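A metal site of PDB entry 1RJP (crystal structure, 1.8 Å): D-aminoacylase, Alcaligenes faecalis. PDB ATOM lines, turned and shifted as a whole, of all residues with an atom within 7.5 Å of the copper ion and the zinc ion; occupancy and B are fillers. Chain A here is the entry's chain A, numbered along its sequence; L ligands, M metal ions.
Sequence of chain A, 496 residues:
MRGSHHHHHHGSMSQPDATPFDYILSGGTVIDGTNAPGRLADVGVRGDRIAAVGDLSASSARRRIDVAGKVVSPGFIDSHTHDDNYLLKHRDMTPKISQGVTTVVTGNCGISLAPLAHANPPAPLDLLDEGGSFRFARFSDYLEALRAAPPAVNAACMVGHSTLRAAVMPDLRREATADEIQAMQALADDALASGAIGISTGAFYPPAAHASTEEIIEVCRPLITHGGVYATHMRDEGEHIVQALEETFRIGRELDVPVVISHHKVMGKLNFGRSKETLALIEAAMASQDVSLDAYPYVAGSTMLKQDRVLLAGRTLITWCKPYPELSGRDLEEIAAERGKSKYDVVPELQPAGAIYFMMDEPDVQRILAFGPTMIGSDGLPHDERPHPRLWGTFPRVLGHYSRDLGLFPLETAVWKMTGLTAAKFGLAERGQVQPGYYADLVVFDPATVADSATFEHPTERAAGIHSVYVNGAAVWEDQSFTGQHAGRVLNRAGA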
ATOM      1  N   HIS A  80      27.455 -14.931  17.581  1.00  0.00           N
ATOM      2  CA  HIS A  80      26.337 -15.403  18.397  1.00  0.00           C
ATOM      3  C   HIS A  80      26.109 -16.902  18.295  1.00  0.00           C
ATOM      4  O   HIS A  80      25.406 -17.363  17.387  1.00  0.00           O
ATOM      5  CB  HIS A  80      25.038 -14.717  17.984  1.00  0.00           C
ATOM      6  CG  HIS A  80      23.923 -14.937  18.955  1.00  0.00           C
ATOM      7  ND1 HIS A  80      23.617 -14.019  19.949  1.00  0.00           N
ATOM      8  CD2 HIS A  80      23.143 -16.011  19.172  1.00  0.00           C
ATOM      9  CE1 HIS A  80      22.694 -14.539  20.737  1.00  0.00           C
ATOM     10  NE2 HIS A  80      22.386 -15.744  20.293  1.00  0.00           N
ATOM     11  N   THR A  81      26.696 -17.666  19.214  1.00  0.00           N
ATOM     12  CA  THR A  81      26.528 -19.108  19.176  1.00  0.00           C
ATOM     13  C   THR A  81      26.012 -19.673  20.485  1.00  0.00           C
ATOM     14  O   THR A  81      26.037 -19.025  21.535  1.00  0.00           O
ATOM     15  CB  THR A  81      27.859 -19.874  18.936  1.00  0.00           C
ATOM     16  OG1 THR A  81      28.635 -19.913  20.158  1.00  0.00           O
ATOM     17  CG2 THR A  81      28.680 -19.207  17.866  1.00  0.00           C
ATOM     18  N   HIS A  82      25.576 -20.912  20.378  1.00  0.00           N
ATOM     19  CA  HIS A  82      25.156 -21.699  21.531  1.00  0.00           C
ATOM     20  C   HIS A  82      25.958 -22.981  21.416  1.00  0.00           C
ATOM     21  O   HIS A  82      25.441 -24.082  21.565  1.00  0.00           O
ATOM     22  CB  HIS A  82      23.648 -21.919  21.493  1.00  0.00           C
ATOM     23  CG  HIS A  82      22.879 -20.696  21.899  1.00  0.00           C
ATOM     24  ND1 HIS A  82      22.924 -20.197  23.183  1.00  0.00           N
ATOM     25  CD2 HIS A  82      22.138 -19.823  21.172  1.00  0.00           C
ATOM     26  CE1 HIS A  82      22.242 -19.060  23.225  1.00  0.00           C
ATOM     27  NE2 HIS A  82      21.764 -18.814  22.013  1.00  0.00           N
ATOM     28  N   GLY A 107      27.896 -18.768  25.272  1.00  0.00           N
ATOM     29  CA  GLY A 107      27.209 -18.294  26.473  1.00  0.00           C
ATOM     30  C   GLY A 107      26.321 -17.082  26.243  1.00  0.00           C
ATOM     31  O   GLY A 107      26.383 -16.091  27.001  1.00  0.00           O
ATOM     32  N   ASN A 108      25.481 -17.174  25.217  1.00  0.00           N
ATOM     33  CA  ASN A 108      24.578 -16.085  24.835  1.00  0.00           C
ATOM     34  C   ASN A 108      23.155 -16.177  25.388  1.00  0.00           C
ATOM     35  O   ASN A 108      22.711 -17.230  25.846  1.00  0.00           O
ATOM     36  CB  ASN A 108      24.504 -16.003  23.309  1.00  0.00           C
ATOM     37  CG  ASN A 108      25.758 -15.429  22.687  1.00  0.00           C
ATOM     38  OD1 ASN A 108      26.665 -16.163  22.207  1.00  0.00           O
ATOM     39  ND2 ASN A 108      25.852 -14.118  22.711  1.00  0.00           N
ATOM     40  N   CYS A 109      22.438 -15.053  25.318  1.00  0.00           N
ATOM     41  CA  CYS A 109      21.039 -14.974  25.735  1.00  0.00           C
ATOM     42  C   CYS A 109      20.757 -15.400  27.173  1.00  0.00           C
ATOM     43  O   CYS A 109      19.646 -15.859  27.499  1.00  0.00           O
ATOM     44  CB  CYS A 109      20.190 -15.781  24.752  1.00  0.00           C
ATOM     45  SG  CYS A 109      20.465 -15.282  23.035  1.00  0.00           S
ATOM     46  N   GLY A 110      21.761 -15.230  28.024  1.00  0.00           N
ATOM     47  CA  GLY A 110      21.646 -15.593  29.415  1.00  0.00           C
ATOM     48  C   GLY A 110      21.916 -17.066  29.680  1.00  0.00           C
ATOM     49  O   GLY A 110      21.902 -17.494  30.826  1.00  0.00           O
ATOM     50  N   ILE A 111      22.193 -17.804  28.608  1.00  0.00           N
ATOM     51  CA  ILE A 111      22.417 -19.251  28.660  1.00  0.00           C
ATOM     52  C   ILE A 111      23.877 -19.705  28.529  1.00  0.00           C
ATOM     53  O   ILE A 111      24.414 -19.689  27.426  1.00  0.00           O
ATOM     54  CB  ILE A 111      21.637 -19.944  27.499  1.00  0.00           C
ATOM     55  CG1 ILE A 111      20.182 -19.500  27.517  1.00  0.00           C
ATOM     56  CG2 ILE A 111      21.748 -21.471  27.605  1.00  0.00           C
ATOM     57  CD1 ILE A 111      19.373 -19.971  26.306  1.00  0.00           C
ATOM     58  N   LEU A 127      18.729 -26.243  25.725  1.00  0.00           N
ATOM     59  CA  LEU A 127      19.209 -26.208  24.328  1.00  0.00           C
ATOM     60  C   LEU A 127      20.684 -26.653  24.240  1.00  0.00           C
ATOM     61  O   LEU A 127      21.130 -27.073  23.181  1.00  0.00           O
ATOM     62  CB  LEU A 127      19.062 -24.807  23.730  1.00  0.00           C
ATOM     63  CG  LEU A 127      17.635 -24.307  23.436  1.00  0.00           C
ATOM     64  CD1 LEU A 127      17.740 -22.879  22.964  1.00  0.00           C
ATOM     65  CD2 LEU A 127      16.936 -25.190  22.378  1.00  0.00           C
ATOM     66  N   THR A 201      22.401 -11.834  29.111  1.00  0.00           N
ATOM     67  CA  THR A 201      21.086 -11.933  29.751  1.00  0.00           C
ATOM     68  C   THR A 201      20.049 -12.297  28.660  1.00  0.00           C
ATOM     69  O   THR A 201      20.268 -12.086  27.454  1.00  0.00           O
ATOM     70  CB  THR A 201      20.640 -10.585  30.396  1.00  0.00           C
ATOM     71  OG1 THR A 201      20.466  -9.611  29.367  1.00  0.00           O
ATOM     72  CG2 THR A 201      21.679 -10.076  31.388  1.00  0.00           C
ATOM     73  N   GLY A 202      18.931 -12.868  29.091  1.00  0.00           N
ATOM     74  CA  GLY A 202      17.840 -13.263  28.219  1.00  0.00           C
ATOM     75  C   GLY A 202      16.564 -13.196  29.042  1.00  0.00           C
ATOM     76  O   GLY A 202      15.913 -14.229  29.283  1.00  0.00           O
ATOM     77  N   PHE A 204      13.755 -12.416  28.309  1.00  0.00           N
ATOM     78  CA  PHE A 204      12.606 -12.853  27.523  1.00  0.00           C
ATOM     79  C   PHE A 204      12.182 -14.228  28.021  1.00  0.00           C
ATOM     80  O   PHE A 204      10.994 -14.569  28.016  1.00  0.00           O
ATOM     81  CB  PHE A 204      13.035 -12.952  26.054  1.00  0.00           C
ATOM     82  CG  PHE A 204      12.063 -13.692  25.183  1.00  0.00           C
ATOM     83  CD1 PHE A 204      10.869 -13.096  24.768  1.00  0.00           C
ATOM     84  CD2 PHE A 204      12.370 -14.979  24.718  1.00  0.00           C
ATOM     85  CE1 PHE A 204       9.995 -13.742  23.886  1.00  0.00           C
ATOM     86  CE2 PHE A 204      11.495 -15.649  23.831  1.00  0.00           C
ATOM     87  CZ  PHE A 204      10.301 -15.015  23.415  1.00  0.00           C
ATOM     88  N   TYR A 205      13.149 -15.030  28.455  1.00  0.00           N
ATOM     89  CA  TYR A 205      12.883 -16.392  28.892  1.00  0.00           C
ATOM     90  C   TYR A 205      12.416 -16.587  30.345  1.00  0.00           C
ATOM     91  O   TYR A 205      12.751 -15.809  31.250  1.00  0.00           O
ATOM     92  CB  TYR A 205      14.114 -17.259  28.605  1.00  0.00           C
ATOM     93  CG  TYR A 205      14.412 -17.394  27.129  1.00  0.00           C
ATOM     94  CD1 TYR A 205      13.542 -18.069  26.269  1.00  0.00           C
ATOM     95  CD2 TYR A 205      15.571 -16.821  26.586  1.00  0.00           C
ATOM     96  CE1 TYR A 205      13.821 -18.175  24.898  1.00  0.00           C
ATOM     97  CE2 TYR A 205      15.856 -16.925  25.221  1.00  0.00           C
ATOM     98  CZ  TYR A 205      14.981 -17.613  24.390  1.00  0.00           C
ATOM     99  OH  TYR A 205      15.301 -17.751  23.048  1.00  0.00           O
ATOM    100  N   THR A 232      22.885  -9.155  25.148  1.00  0.00           N
ATOM    101  CA  THR A 232      21.512  -9.405  25.523  1.00  0.00           C
ATOM    102  C   THR A 232      20.498  -9.869  24.483  1.00  0.00           C
ATOM    103  O   THR A 232      20.496  -9.417  23.346  1.00  0.00           O
ATOM    104  CB  THR A 232      20.917  -8.134  26.216  1.00  0.00           C
ATOM    105  OG1 THR A 232      19.555  -8.384  26.611  1.00  0.00           O
ATOM    106  CG2 THR A 232      20.935  -6.917  25.256  1.00  0.00           C
ATOM    107  N   HIS A 233      19.660 -10.809  24.898  1.00  0.00           N
ATOM    108  CA  HIS A 233      18.531 -11.227  24.097  1.00  0.00           C
ATOM    109  C   HIS A 233      17.523 -10.302  24.817  1.00  0.00           C
ATOM    110  O   HIS A 233      17.139 -10.544  25.972  1.00  0.00           O
ATOM    111  CB  HIS A 233      18.212 -12.703  24.312  1.00  0.00           C
ATOM    112  CG  HIS A 233      16.927 -13.138  23.665  1.00  0.00           C
ATOM    113  ND1 HIS A 233      16.767 -14.375  23.082  1.00  0.00           N
ATOM    114  CD2 HIS A 233      15.730 -12.500  23.537  1.00  0.00           C
ATOM    115  CE1 HIS A 233      15.536 -14.488  22.628  1.00  0.00           C
ATOM    116  NE2 HIS A 233      14.884 -13.366  22.896  1.00  0.00           N
ATOM    117  N   MET A 234      17.134  -9.218  24.162  1.00  0.00           N
ATOM    118  CA  MET A 234      16.236  -8.244  24.764  1.00  0.00           C
ATOM    119  C   MET A 234      14.934  -8.820  25.330  1.00  0.00           C
ATOM    120  O   MET A 234      14.417  -9.850  24.874  1.00  0.00           O
ATOM    121  CB  MET A 234      15.976  -7.104  23.776  1.00  0.00           C
ATOM    122  CG  MET A 234      17.279  -6.367  23.408  1.00  0.00           C
ATOM    123  SD  MET A 234      16.995  -4.809  22.500  1.00  0.00           S
ATOM    124  CE  MET A 234      16.231  -5.411  20.978  1.00  0.00           C
ATOM    125  N   GLU A 237      11.026  -8.485  21.625  1.00  0.00           N
ATOM    126  CA  GLU A 237      11.478  -8.091  20.292  1.00  0.00           C
ATOM    127  C   GLU A 237      10.320  -7.838  19.352  1.00  0.00           C
ATOM    128  O   GLU A 237      10.460  -7.937  18.137  1.00  0.00           O
ATOM    129  CB  GLU A 237      12.391  -9.172  19.704  1.00  0.00           C
ATOM    130  CG  GLU A 237      13.686  -9.382  20.482  1.00  0.00           C
ATOM    131  CD  GLU A 237      14.621 -10.381  19.801  1.00  0.00           C
ATOM    132  OE1 GLU A 237      14.172 -11.520  19.554  1.00  0.00           O
ATOM    133  OE2 GLU A 237      15.787 -10.034  19.510  1.00  0.00           O
ATOM    134  N   SER A 262      21.703  -8.880  20.774  1.00  0.00           N
ATOM    135  CA  SER A 262      21.729 -10.135  20.015  1.00  0.00           C
ATOM    136  C   SER A 262      20.606 -10.313  19.020  1.00  0.00           C
ATOM    137  O   SER A 262      19.492  -9.835  19.250  1.00  0.00           O
ATOM    138  CB  SER A 262      21.700 -11.323  20.976  1.00  0.00           C
ATOM    139  OG  SER A 262      22.784 -11.288  21.873  1.00  0.00           O
ATOM    140  N   HIS A 263      20.904 -11.033  17.931  1.00  0.00           N
ATOM    141  CA  HIS A 263      19.959 -11.353  16.858  1.00  0.00           C
ATOM    142  C   HIS A 263      18.820 -10.318  16.694  1.00  0.00           C
ATOM    143  O   HIS A 263      17.651 -10.623  16.890  1.00  0.00           O
ATOM    144  CB  HIS A 263      19.382 -12.771  17.058  1.00  0.00           C
ATOM    145  CG  HIS A 263      18.866 -13.053  18.448  1.00  0.00           C
ATOM    146  ND1 HIS A 263      17.911 -12.282  19.063  1.00  0.00           N
ATOM    147  CD2 HIS A 263      19.141 -14.069  19.315  1.00  0.00           C
ATOM    148  CE1 HIS A 263      17.610 -12.801  20.246  1.00  0.00           C
ATOM    149  NE2 HIS A 263      18.345 -13.886  20.422  1.00  0.00           N
ATOM    150  N   LYS A 265      15.898  -8.076  15.439  1.00  0.00           N
ATOM    151  CA  LYS A 265      14.773  -8.362  14.543  1.00  0.00           C
ATOM    152  C   LYS A 265      13.555  -7.610  15.057  1.00  0.00           C
ATOM    153  O   LYS A 265      13.579  -7.020  16.134  1.00  0.00           O
ATOM    154  CB  LYS A 265      14.430  -9.859  14.620  1.00  0.00           C
ATOM    155  CG  LYS A 265      13.810 -10.243  15.999  1.00  0.00           C
ATOM    156  CD  LYS A 265      13.387 -11.731  16.116  1.00  0.00           C
ATOM    157  CE  LYS A 265      14.590 -12.681  16.106  1.00  0.00           C
ATOM    158  NZ  LYS A 265      15.449 -12.554  17.332  1.00  0.00           N
ATOM    159  N   TYR A 296      21.209 -12.913  12.198  1.00  0.00           N
ATOM    160  CA  TYR A 296      21.353 -14.058  11.301  1.00  0.00           C
ATOM    161  C   TYR A 296      20.533 -13.713  10.042  1.00  0.00           C
ATOM    162  O   TYR A 296      19.544 -12.988  10.112  1.00  0.00           O
ATOM    163  CB  TYR A 296      20.894 -15.361  11.967  1.00  0.00           C
ATOM    164  CG  TYR A 296      19.535 -15.321  12.626  1.00  0.00           C
ATOM    165  CD1 TYR A 296      18.362 -15.529  11.893  1.00  0.00           C
ATOM    166  CD2 TYR A 296      19.428 -15.125  13.998  1.00  0.00           C
ATOM    167  CE1 TYR A 296      17.121 -15.550  12.523  1.00  0.00           C
ATOM    168  CE2 TYR A 296      18.192 -15.138  14.650  1.00  0.00           C
ATOM    169  CZ  TYR A 296      17.046 -15.349  13.904  1.00  0.00           C
ATOM    170  OH  TYR A 296      15.831 -15.340  14.570  1.00  0.00           O
ATOM    171  N   SER A 302      14.433 -19.594  16.091  1.00  0.00           N
ATOM    172  CA  SER A 302      14.389 -20.924  16.655  1.00  0.00           C
ATOM    173  C   SER A 302      14.847 -20.886  18.098  1.00  0.00           C
ATOM    174  O   SER A 302      15.828 -20.217  18.433  1.00  0.00           O
ATOM    175  CB  SER A 302      15.312 -21.859  15.863  1.00  0.00           C
ATOM    176  OG  SER A 302      15.176 -23.213  16.274  1.00  0.00           O
ATOM    177  N   THR A 303      14.128 -21.591  18.956  1.00  0.00           N
ATOM    178  CA  THR A 303      14.502 -21.698  20.369  1.00  0.00           C
ATOM    179  C   THR A 303      13.579 -22.736  20.990  1.00  0.00           C
ATOM    180  O   THR A 303      13.017 -23.583  20.298  1.00  0.00           O
ATOM    181  CB  THR A 303      14.428 -20.312  21.125  1.00  0.00           C
ATOM    182  OG1 THR A 303      14.855 -20.464  22.482  1.00  0.00           O
ATOM    183  CG2 THR A 303      13.029 -19.763  21.127  1.00  0.00           C
ATOM    184  N   ASP A 379      23.440 -18.084  15.411  1.00  0.00           N
ATOM    185  CA  ASP A 379      22.436 -18.486  16.399  1.00  0.00           C
ATOM    186  C   ASP A 379      22.098 -19.956  16.172  1.00  0.00           C
ATOM    187  O   ASP A 379      20.976 -20.400  16.392  1.00  0.00           O
ATOM    188  CB  ASP A 379      21.164 -17.623  16.305  1.00  0.00           C
ATOM    189  CG  ASP A 379      20.352 -17.626  17.610  1.00  0.00           C
ATOM    190  OD1 ASP A 379      20.743 -18.312  18.578  1.00  0.00           O
ATOM    191  OD2 ASP A 379      19.328 -16.926  17.684  1.00  0.00           O
ATOM    192  N   GLY A 380      23.086 -20.729  15.711  1.00  0.00           N
ATOM    193  CA  GLY A 380      22.832 -22.142  15.519  1.00  0.00           C
ATOM    194  C   GLY A 380      22.583 -22.881  16.835  1.00  0.00           C
ATOM    195  O   GLY A 380      23.215 -22.589  17.853  1.00  0.00           O
ATOM    196  N   LEU A 381      21.643 -23.814  16.826  1.00  0.00           N
ATOM    197  CA  LEU A 381      21.313 -24.628  18.014  1.00  0.00           C
ATOM    198  C   LEU A 381      21.789 -26.018  17.560  1.00  0.00           C
ATOM    199  O   LEU A 381      21.014 -26.802  17.006  1.00  0.00           O
ATOM    200  CB  LEU A 381      19.802 -24.557  18.263  1.00  0.00           C
ATOM    201  CG  LEU A 381      19.308 -23.103  18.329  1.00  0.00           C
ATOM    202  CD1 LEU A 381      17.820 -23.052  18.687  1.00  0.00           C
ATOM    203  CD2 LEU A 381      20.121 -22.324  19.366  1.00  0.00           C
ATOM    204  N   ARG A 390      20.368 -22.153   9.651  1.00  0.00           N
ATOM    205  CA  ARG A 390      21.361 -21.128   9.989  1.00  0.00           C
ATOM    206  C   ARG A 390      22.572 -21.816  10.648  1.00  0.00           C
ATOM    207  O   ARG A 390      23.712 -21.343  10.569  1.00  0.00           O
ATOM    208  CB  ARG A 390      20.751 -20.088  10.945  1.00  0.00           C
ATOM    209  CG  ARG A 390      20.276 -20.632  12.308  1.00  0.00           C
ATOM    210  CD  ARG A 390      19.262 -19.681  12.975  1.00  0.00           C
ATOM    211  NE  ARG A 390      19.096 -19.953  14.401  1.00  0.00           N
ATOM    212  CZ  ARG A 390      18.234 -19.328  15.197  1.00  0.00           C
ATOM    213  NH1 ARG A 390      17.439 -18.371  14.717  1.00  0.00           N
ATOM    214  NH2 ARG A 390      18.165 -19.660  16.474  1.00  0.00           N
HETATM  215  C1  LIG L   1      18.195 -17.699  21.181  1.00  0.00           C
HETATM  216  O1  LIG L   1      17.661 -17.113  22.157  1.00  0.00           O
HETATM  217  O2  LIG L   1      18.969 -17.126  20.383  1.00  0.00           O
HETATM  218  C2  LIG L   1      17.972 -19.189  21.020  1.00  0.00           C
HETATM  219 CU    CU M   1      21.274 -16.903  21.631  1.00  0.00          CU
HETATM  220 ZN    ZN M   2      18.362 -15.241  22.041  1.00  0.00          ZN
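O of Thr 81 lies close to OD1 of Asn 108 (3.0 Å). A ring nitrogen (ND1) of His 263 lies within hydrogen-bond range of the side-chain carboxylate of Glu 237. O of His 263 is in hydrogen-bond range of NZ of Lys 265 (3.0 Å). N of Asp 379 lies within hydrogen-bond range of O of His 80 (2.9 Å). A ring nitrogen (ND1) of His 80 lies within hydrogen-bond range of the side-chain hydroxyl (OG) of Ser 262 (3.4 Å). OD2 of Asp 379 lies within salt-bridge range of NH2 of Arg 390 (3.2 Å). The backbone carbonyl oxygen (O) of Thr 201 lies within hydrogen-bond range of the backbone NH (N) of His 233 (2.9 Å). The backbone carbonyl oxygen (O) of Cys 109 lies close to the backbone NH (N) of Gly 202 (3.5 Å).
Residues that only touch the copper ion: Asp 379 (3.4 Å) and Asn 108 (3.7 Å).
The nearest printed residue that does not touch the zinc ion is Tyr 205 (4.1 Å).
The copper ion is bound by a ring nitrogen (NE2) of His 82 (2.0 Å), a ring nitrogen (NE2) of His 80 (2.1 Å) and the side-chain sulfur (SG) of Cys 109 (2.3 Å). The copper ion has three donor atoms within binding distance. Slightly farther from the copper ion lies O2 of the ligand (2.6 Å).
The zinc ion is bound by O1 of the ligand (2.0 Å), ND1 of His 233 (2.1 Å), NE2 of His 263 (2.1 Å), SG of Cys 109 (2.3 Å) and O2 of the ligand (2.6 Å).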
